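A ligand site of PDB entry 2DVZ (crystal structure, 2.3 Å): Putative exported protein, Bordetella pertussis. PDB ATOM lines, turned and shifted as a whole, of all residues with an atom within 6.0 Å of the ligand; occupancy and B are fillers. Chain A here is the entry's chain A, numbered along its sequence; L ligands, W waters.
Merely in contact with the ligand: Phe 27 (3.5 Å), Gly 31 (3.6 Å), Ser 32 (3.5 Å), Thr 83 (3.6 Å), Val 84 (3.8 Å), Val 154 (3.1 Å), Leu 155 (3.4 Å) and Gly 177 (3.4 Å). Hydrophobic or aromatic side chains that line the ligand: Phe 27, Val 154, Leu 155 and Tyr 243.
The side-chain amide oxygen (OD1) of Asn 196 sits close to the side-chain hydroxyl (OH) of Tyr 243. The side-chain hydroxyl (OG) of Ser 32 is in hydrogen-bond range of the side-chain hydroxyl (OG) of Ser 199, at 3.1 Å. The backbone NH (N) of Ser 85 sits close to the side-chain hydroxyl (OG1) of Thr 83 (3.4 Å). The backbone carbonyl oxygen of Asn 196 sits at hydrogen-bond distance from the side-chain hydroxyl of Ser 199 (3.4 Å). The side-chain hydroxyl (OG) of Ser 85 sits at hydrogen-bond distance from the backbone NH (N) of Val 154, at 2.7 Å. The backbone carbonyl oxygen of Asn 196 is in hydrogen-bond range of the side-chain hydroxyl of Ser 32 (3.3 Å). The side-chain hydroxyl (OG) of Ser 178 sits at hydrogen-bond distance from the side-chain carboxylate (OD1) of Asp 195, 2.7 Å away. The side-chain hydroxyl (OG1) of Thr 83 lies within hydrogen-bond range of the side-chain hydroxyl (OG1) of Thr 86 (2.7 Å).
Water W2 lies within hydrogen-bond range of an oxygen (O2) of the ligand (2.7 Å), the backbone carbonyl oxygen (O) of Ala 28 (2.8 Å), the backbone NH (N) of Asp 34 (3.1 Å) and the backbone NH (N) of Gly 31 (3.2 Å). Water W3 lies within hydrogen-bond range of an oxygen (O1) of the ligand (2.7 Å), the backbone NH of Val 84 (2.8 Å) and the backbone carbonyl oxygen of Trp 242 (2.9 Å). Water W4 lies within hydrogen-bond range of the side-chain amide oxygen of Asn 196 (2.5 Å), the side-chain hydroxyl of Ser 32 (2.9 Å), the side-chain carboxylate of Asp 195 (3.0 Å), the side-chain hydroxyl of Ser 199 (3.1 Å) and the side-chain hydroxyl of Ser 178 (3.3 Å).
OD1 of Asn 196 sits close to O1 of the ligand, at 3.4 Å. The backbone NH (N) of Ser 178 is in hydrogen-bond range of an oxygen (O3) of the ligand, at 2.9 Å. O2 of the ligand lies within hydrogen-bond range of N of Thr 33. OG of Ser 149 sits at hydrogen-bond distance from N1 of the ligand (2.7 Å). An oxygen (O2) of the ligand sits at hydrogen-bond distance from the side-chain hydroxyl (OG1) of Thr 33 (2.6 Å). The side-chain hydroxyl (OH) of Tyr 243 lies within hydrogen-bond range of an oxygen (O1) of the ligand (2.6 Å). The side-chain hydroxyl of Ser 85 is in hydrogen-bond range of an oxygen (O4) of the ligand. N of Ser 85 lies within hydrogen-bond range of O4 of the ligand (3.2 Å).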
ATOM      1  N   VAL A  25      13.441 -20.681  11.158  1.00  0.00           N
ATOM      2  CA  VAL A  25      14.135 -21.960  11.119  1.00  0.00           C
ATOM      3  C   VAL A  25      15.579 -21.713  10.649  1.00  0.00           C
ATOM      4  O   VAL A  25      15.811 -21.339   9.488  1.00  0.00           O
ATOM      5  CB  VAL A  25      13.321 -22.981  10.240  1.00  0.00           C
ATOM      6  CG1 VAL A  25      14.136 -24.245   9.904  1.00  0.00           C
ATOM      7  CG2 VAL A  25      12.051 -23.329  10.949  1.00  0.00           C
ATOM      8  N   PHE A  27      17.851 -23.315   9.460  1.00  0.00           N
ATOM      9  CA  PHE A  27      18.394 -24.279   8.507  1.00  0.00           C
ATOM     10  C   PHE A  27      17.593 -24.224   7.221  1.00  0.00           C
ATOM     11  O   PHE A  27      16.462 -23.772   7.198  1.00  0.00           O
ATOM     12  CB  PHE A  27      18.380 -25.687   9.098  1.00  0.00           C
ATOM     13  CG  PHE A  27      19.428 -25.908  10.101  1.00  0.00           C
ATOM     14  CD1 PHE A  27      20.769 -26.114   9.709  1.00  0.00           C
ATOM     15  CD2 PHE A  27      19.129 -25.858  11.463  1.00  0.00           C
ATOM     16  CE1 PHE A  27      21.776 -26.280  10.635  1.00  0.00           C
ATOM     17  CE2 PHE A  27      20.151 -26.037  12.411  1.00  0.00           C
ATOM     18  CZ  PHE A  27      21.475 -26.243  11.994  1.00  0.00           C
ATOM     19  N   ALA A  28      18.193 -24.738   6.153  1.00  0.00           N
ATOM     20  CA  ALA A  28      17.561 -24.832   4.834  1.00  0.00           C
ATOM     21  C   ALA A  28      16.278 -25.679   4.878  1.00  0.00           C
ATOM     22  O   ALA A  28      16.088 -26.488   5.796  1.00  0.00           O
ATOM     23  CB  ALA A  28      18.573 -25.454   3.844  1.00  0.00           C
ATOM     24  N   GLY A  30      13.671 -28.606   4.320  1.00  0.00           N
ATOM     25  CA  GLY A  30      13.683 -30.030   4.081  1.00  0.00           C
ATOM     26  C   GLY A  30      14.652 -30.751   4.976  1.00  0.00           C
ATOM     27  O   GLY A  30      14.955 -31.920   4.724  1.00  0.00           O
ATOM     28  N   GLY A  31      15.172 -30.081   5.996  1.00  0.00           N
ATOM     29  CA  GLY A  31      15.891 -30.781   7.067  1.00  0.00           C
ATOM     30  C   GLY A  31      14.881 -31.105   8.156  1.00  0.00           C
ATOM     31  O   GLY A  31      13.700 -30.809   7.994  1.00  0.00           O
ATOM     32  N   SER A  32      15.334 -31.697   9.257  1.00  0.00           N
ATOM     33  CA  SER A  32      14.433 -32.052  10.337  1.00  0.00           C
ATOM     34  C   SER A  32      13.853 -30.812  11.047  1.00  0.00           C
ATOM     35  O   SER A  32      12.685 -30.822  11.454  1.00  0.00           O
ATOM     36  CB  SER A  32      15.140 -32.986  11.352  1.00  0.00           C
ATOM     37  OG  SER A  32      15.663 -34.136  10.698  1.00  0.00           O
ATOM     38  N   THR A  33      14.673 -29.771  11.252  1.00  0.00           N
ATOM     39  CA  THR A  33      14.194 -28.525  11.843  1.00  0.00           C
ATOM     40  C   THR A  33      13.010 -27.986  11.060  1.00  0.00           C
ATOM     41  O   THR A  33      11.947 -27.771  11.635  1.00  0.00           O
ATOM     42  CB  THR A  33      15.293 -27.435  11.874  1.00  0.00           C
ATOM     43  OG1 THR A  33      16.561 -28.039  12.194  1.00  0.00           O
ATOM     44  CG2 THR A  33      14.948 -26.365  12.888  1.00  0.00           C
ATOM     45  N   ASP A  34      13.189 -27.790   9.763  1.00  0.00           N
ATOM     46  CA  ASP A  34      12.093 -27.431   8.855  1.00  0.00           C
ATOM     47  C   ASP A  34      10.886 -28.395   8.900  1.00  0.00           C
ATOM     48  O   ASP A  34       9.728 -27.957   8.971  1.00  0.00           O
ATOM     49  CB  ASP A  34      12.642 -27.358   7.436  1.00  0.00           C
ATOM     50  CG  ASP A  34      11.680 -26.687   6.454  1.00  0.00           C
ATOM     51  OD1 ASP A  34      11.273 -25.523   6.715  1.00  0.00           O
ATOM     52  OD2 ASP A  34      11.386 -27.308   5.403  1.00  0.00           O
ATOM     53  N   THR A  83      17.680 -25.742  18.308  1.00  0.00           N
ATOM     54  CA  THR A  83      18.260 -26.978  17.803  1.00  0.00           C
ATOM     55  C   THR A  83      19.508 -27.159  18.609  1.00  0.00           C
ATOM     56  O   THR A  83      20.001 -26.195  19.202  1.00  0.00           O
ATOM     57  CB  THR A  83      18.661 -26.863  16.321  1.00  0.00           C
ATOM     58  OG1 THR A  83      19.713 -25.907  16.211  1.00  0.00           O
ATOM     59  CG2 THR A  83      17.477 -26.461  15.427  1.00  0.00           C
ATOM     60  N   VAL A  84      20.046 -28.378  18.639  1.00  0.00           N
ATOM     61  CA  VAL A  84      21.280 -28.614  19.360  1.00  0.00           C
ATOM     62  C   VAL A  84      22.469 -27.898  18.693  1.00  0.00           C
ATOM     63  O   VAL A  84      23.423 -27.531  19.367  1.00  0.00           O
ATOM     64  CB  VAL A  84      21.542 -30.150  19.642  1.00  0.00           C
ATOM     65  CG1 VAL A  84      22.862 -30.333  20.380  1.00  0.00           C
ATOM     66  CG2 VAL A  84      20.429 -30.758  20.495  1.00  0.00           C
ATOM     67  N   SER A  85      22.405 -27.703  17.382  1.00  0.00           N
ATOM     68  CA  SER A  85      23.433 -26.949  16.678  1.00  0.00           C
ATOM     69  C   SER A  85      23.483 -25.520  17.235  1.00  0.00           C
ATOM     70  O   SER A  85      24.544 -25.024  17.593  1.00  0.00           O
ATOM     71  CB  SER A  85      23.164 -26.918  15.162  1.00  0.00           C
ATOM     72  OG  SER A  85      23.393 -28.197  14.579  1.00  0.00           O
ATOM     73  N   THR A  86      22.324 -24.900  17.338  1.00  0.00           N
ATOM     74  CA  THR A  86      22.253 -23.470  17.692  1.00  0.00           C
ATOM     75  C   THR A  86      22.377 -23.210  19.203  1.00  0.00           C
ATOM     76  O   THR A  86      22.880 -22.167  19.607  1.00  0.00           O
ATOM     77  CB  THR A  86      21.013 -22.782  17.071  1.00  0.00           C
ATOM     78  OG1 THR A  86      19.820 -23.497  17.431  1.00  0.00           O
ATOM     79  CG2 THR A  86      21.128 -22.736  15.532  1.00  0.00           C
ATOM     80  N   SER A 149      24.980 -30.981   8.248  1.00  0.00           N
ATOM     81  CA  SER A 149      24.119 -29.793   8.097  1.00  0.00           C
ATOM     82  C   SER A 149      24.885 -28.500   8.344  1.00  0.00           C
ATOM     83  O   SER A 149      24.270 -27.455   8.393  1.00  0.00           O
ATOM     84  CB  SER A 149      22.981 -29.865   9.111  1.00  0.00           C
ATOM     85  OG  SER A 149      23.513 -29.808  10.449  1.00  0.00           O
ATOM     86  N   GLY A 153      27.673 -27.335  13.475  1.00  0.00           N
ATOM     87  CA  GLY A 153      26.430 -27.965  13.833  1.00  0.00           C
ATOM     88  C   GLY A 153      26.630 -29.306  14.488  1.00  0.00           C
ATOM     89  O   GLY A 153      27.734 -29.881  14.448  1.00  0.00           O
ATOM     90  N   VAL A 154      25.529 -29.828  15.074  1.00  0.00           N
ATOM     91  CA  VAL A 154      25.549 -31.111  15.750  1.00  0.00           C
ATOM     92  C   VAL A 154      25.914 -32.325  14.875  1.00  0.00           C
ATOM     93  O   VAL A 154      26.428 -33.309  15.386  1.00  0.00           O
ATOM     94  CB  VAL A 154      24.230 -31.381  16.573  1.00  0.00           C
ATOM     95  CG1 VAL A 154      23.085 -31.600  15.687  1.00  0.00           C
ATOM     96  CG2 VAL A 154      24.429 -32.558  17.504  1.00  0.00           C
ATOM     97  N   LEU A 155      25.645 -32.266  13.583  1.00  0.00           N
ATOM     98  CA  LEU A 155      25.903 -33.416  12.729  1.00  0.00           C
ATOM     99  C   LEU A 155      27.376 -33.494  12.317  1.00  0.00           C
ATOM    100  O   LEU A 155      27.884 -34.581  12.132  1.00  0.00           O
ATOM    101  CB  LEU A 155      24.920 -33.456  11.546  1.00  0.00           C
ATOM    102  CG  LEU A 155      23.447 -33.462  12.015  1.00  0.00           C
ATOM    103  CD1 LEU A 155      22.528 -33.186  10.884  1.00  0.00           C
ATOM    104  CD2 LEU A 155      23.089 -34.784  12.719  1.00  0.00           C
ATOM    105  N   LYS A 176      24.376 -26.591   3.708  1.00  0.00           N
ATOM    106  CA  LYS A 176      23.530 -25.532   4.330  1.00  0.00           C
ATOM    107  C   LYS A 176      22.377 -26.036   5.267  1.00  0.00           C
ATOM    108  O   LYS A 176      21.635 -25.231   5.988  1.00  0.00           O
ATOM    109  CB  LYS A 176      23.043 -24.575   3.229  1.00  0.00           C
ATOM    110  CG  LYS A 176      22.769 -23.168   3.694  1.00  0.00           C
ATOM    111  CD  LYS A 176      22.504 -22.266   2.499  1.00  0.00           C
ATOM    112  CE  LYS A 176      22.139 -20.897   2.986  1.00  0.00           C
ATOM    113  NZ  LYS A 176      22.695 -19.828   2.106  1.00  0.00           N
ATOM    114  N   GLY A 177      22.284 -27.356   5.326  1.00  0.00           N
ATOM    115  CA  GLY A 177      21.432 -28.088   6.233  1.00  0.00           C
ATOM    116  C   GLY A 177      21.386 -29.501   5.664  1.00  0.00           C
ATOM    117  O   GLY A 177      21.947 -29.746   4.615  1.00  0.00           O
ATOM    118  N   SER A 178      20.715 -30.415   6.368  1.00  0.00           N
ATOM    119  CA  SER A 178      20.577 -31.803   5.948  1.00  0.00           C
ATOM    120  C   SER A 178      19.756 -31.978   4.661  1.00  0.00           C
ATOM    121  O   SER A 178      19.966 -32.964   3.922  1.00  0.00           O
ATOM    122  CB  SER A 178      19.987 -32.611   7.071  1.00  0.00           C
ATOM    123  OG  SER A 178      20.888 -32.616   8.159  1.00  0.00           O
ATOM    124  N   GLY A 179      18.841 -31.054   4.373  1.00  0.00           N
ATOM    125  CA  GLY A 179      18.127 -31.031   3.089  1.00  0.00           C
ATOM    126  C   GLY A 179      19.050 -31.331   1.906  1.00  0.00           C
ATOM    127  O   GLY A 179      18.901 -32.383   1.250  1.00  0.00           O
ATOM    128  N   ASP A 195      22.812 -37.622  10.016  1.00  0.00           N
ATOM    129  CA  ASP A 195      21.610 -36.821  10.026  1.00  0.00           C
ATOM    130  C   ASP A 195      20.775 -36.988  11.297  1.00  0.00           C
ATOM    131  O   ASP A 195      21.026 -37.890  12.126  1.00  0.00           O
ATOM    132  CB  ASP A 195      20.737 -37.148   8.806  1.00  0.00           C
ATOM    133  CG  ASP A 195      19.778 -36.026   8.450  1.00  0.00           C
ATOM    134  OD1 ASP A 195      19.890 -34.929   9.048  1.00  0.00           O
ATOM    135  OD2 ASP A 195      18.907 -36.239   7.577  1.00  0.00           O
ATOM    136  N   ASN A 196      19.822 -36.060  11.455  1.00  0.00           N
ATOM    137  CA  ASN A 196      18.730 -36.198  12.372  1.00  0.00           C
ATOM    138  C   ASN A 196      17.757 -37.010  11.581  1.00  0.00           C
ATOM    139  O   ASN A 196      17.567 -36.781  10.383  1.00  0.00           O
ATOM    140  CB  ASN A 196      18.126 -34.822  12.765  1.00  0.00           C
ATOM    141  CG  ASN A 196      19.203 -33.686  12.910  1.00  0.00           C
ATOM    142  OD1 ASN A 196      19.208 -32.757  12.103  1.00  0.00           O
ATOM    143  ND2 ASN A 196      20.067 -33.776  13.895  1.00  0.00           N
ATOM    144  N   SER A 199      14.594 -36.158   8.389  1.00  0.00           N
ATOM    145  CA  SER A 199      14.874 -35.786   6.988  1.00  0.00           C
ATOM    146  C   SER A 199      15.382 -36.963   6.145  1.00  0.00           C
ATOM    147  O   SER A 199      15.191 -36.998   4.923  1.00  0.00           O
ATOM    148  CB  SER A 199      15.857 -34.603   6.861  1.00  0.00           C
ATOM    149  OG  SER A 199      16.836 -34.638   7.877  1.00  0.00           O
ATOM    150  N   VAL A 241      18.883 -35.738  19.777  1.00  0.00           N
ATOM    151  CA  VAL A 241      18.735 -34.280  19.801  1.00  0.00           C
ATOM    152  C   VAL A 241      17.260 -33.919  20.137  1.00  0.00           C
ATOM    153  O   VAL A 241      16.493 -34.774  20.659  1.00  0.00           O
ATOM    154  CB  VAL A 241      19.235 -33.638  18.457  1.00  0.00           C
ATOM    155  CG1 VAL A 241      20.696 -33.951  18.258  1.00  0.00           C
ATOM    156  CG2 VAL A 241      18.382 -34.060  17.231  1.00  0.00           C
ATOM    157  N   TRP A 242      16.877 -32.675  19.855  1.00  0.00           N
ATOM    158  CA  TRP A 242      15.534 -32.176  20.115  1.00  0.00           C
ATOM    159  C   TRP A 242      15.316 -30.895  19.330  1.00  0.00           C
ATOM    160  O   TRP A 242      16.273 -30.286  18.821  1.00  0.00           O
ATOM    161  CB  TRP A 242      15.202 -31.970  21.622  1.00  0.00           C
ATOM    162  CG  TRP A 242      16.292 -31.360  22.538  1.00  0.00           C
ATOM    163  CD1 TRP A 242      16.820 -31.936  23.633  1.00  0.00           C
ATOM    164  CD2 TRP A 242      16.942 -30.070  22.413  1.00  0.00           C
ATOM    165  NE1 TRP A 242      17.744 -31.116  24.220  1.00  0.00           N
ATOM    166  CE2 TRP A 242      17.828 -29.945  23.506  1.00  0.00           C
ATOM    167  CE3 TRP A 242      16.850 -28.994  21.498  1.00  0.00           C
ATOM    168  CZ2 TRP A 242      18.683 -28.810  23.698  1.00  0.00           C
ATOM    169  CZ3 TRP A 242      17.710 -27.849  21.671  1.00  0.00           C
ATOM    170  CH2 TRP A 242      18.605 -27.786  22.784  1.00  0.00           C
ATOM    171  N   TYR A 243      14.038 -30.535  19.192  1.00  0.00           N
ATOM    172  CA  TYR A 243      13.587 -29.315  18.543  1.00  0.00           C
ATOM    173  C   TYR A 243      12.584 -28.594  19.428  1.00  0.00           C
ATOM    174  O   TYR A 243      11.676 -29.209  19.945  1.00  0.00           O
ATOM    175  CB  TYR A 243      12.965 -29.642  17.156  1.00  0.00           C
ATOM    176  CG  TYR A 243      14.028 -30.273  16.298  1.00  0.00           C
ATOM    177  CD1 TYR A 243      14.899 -29.461  15.532  1.00  0.00           C
ATOM    178  CD2 TYR A 243      14.239 -31.672  16.310  1.00  0.00           C
ATOM    179  CE1 TYR A 243      15.923 -30.027  14.772  1.00  0.00           C
ATOM    180  CE2 TYR A 243      15.245 -32.246  15.531  1.00  0.00           C
ATOM    181  CZ  TYR A 243      16.103 -31.430  14.786  1.00  0.00           C
ATOM    182  OH  TYR A 243      17.115 -31.992  14.046  1.00  0.00           O
HETATM  183  N1  LIG L   1      21.692 -30.224  12.330  1.00  0.00           N
HETATM  184  C1  LIG L   1      20.476 -29.531  12.793  1.00  0.00           C
HETATM  185  C2  LIG L   1      20.156 -29.835  14.242  1.00  0.00           C
HETATM  186  O1  LIG L   1      19.140 -30.428  14.626  1.00  0.00           O
HETATM  187  C3  LIG L   1      19.311 -29.809  11.849  1.00  0.00           C
HETATM  188  C4  LIG L   1      19.722 -29.695  10.368  1.00  0.00           C
HETATM  189  C5  LIG L   1      18.618 -29.254   9.451  1.00  0.00           C
HETATM  190  O2  LIG L   1      17.506 -29.010   9.979  1.00  0.00           O
HETATM  191  O3  LIG L   1      18.854 -29.116   8.198  1.00  0.00           O
HETATM  192  O4  LIG L   1      20.943 -29.418  15.113  1.00  0.00           O
HETATM  193  O   HOH W   1      17.979 -28.351   5.899  1.00  0.00           O
HETATM  194  O   HOH W   2      15.853 -27.851   8.221  1.00  0.00           O
HETATM  195  O   HOH W   3      18.742 -30.411  17.298  1.00  0.00           O
HETATM  196  O   HOH W   4      18.059 -32.672   9.870  1.00  0.00           O
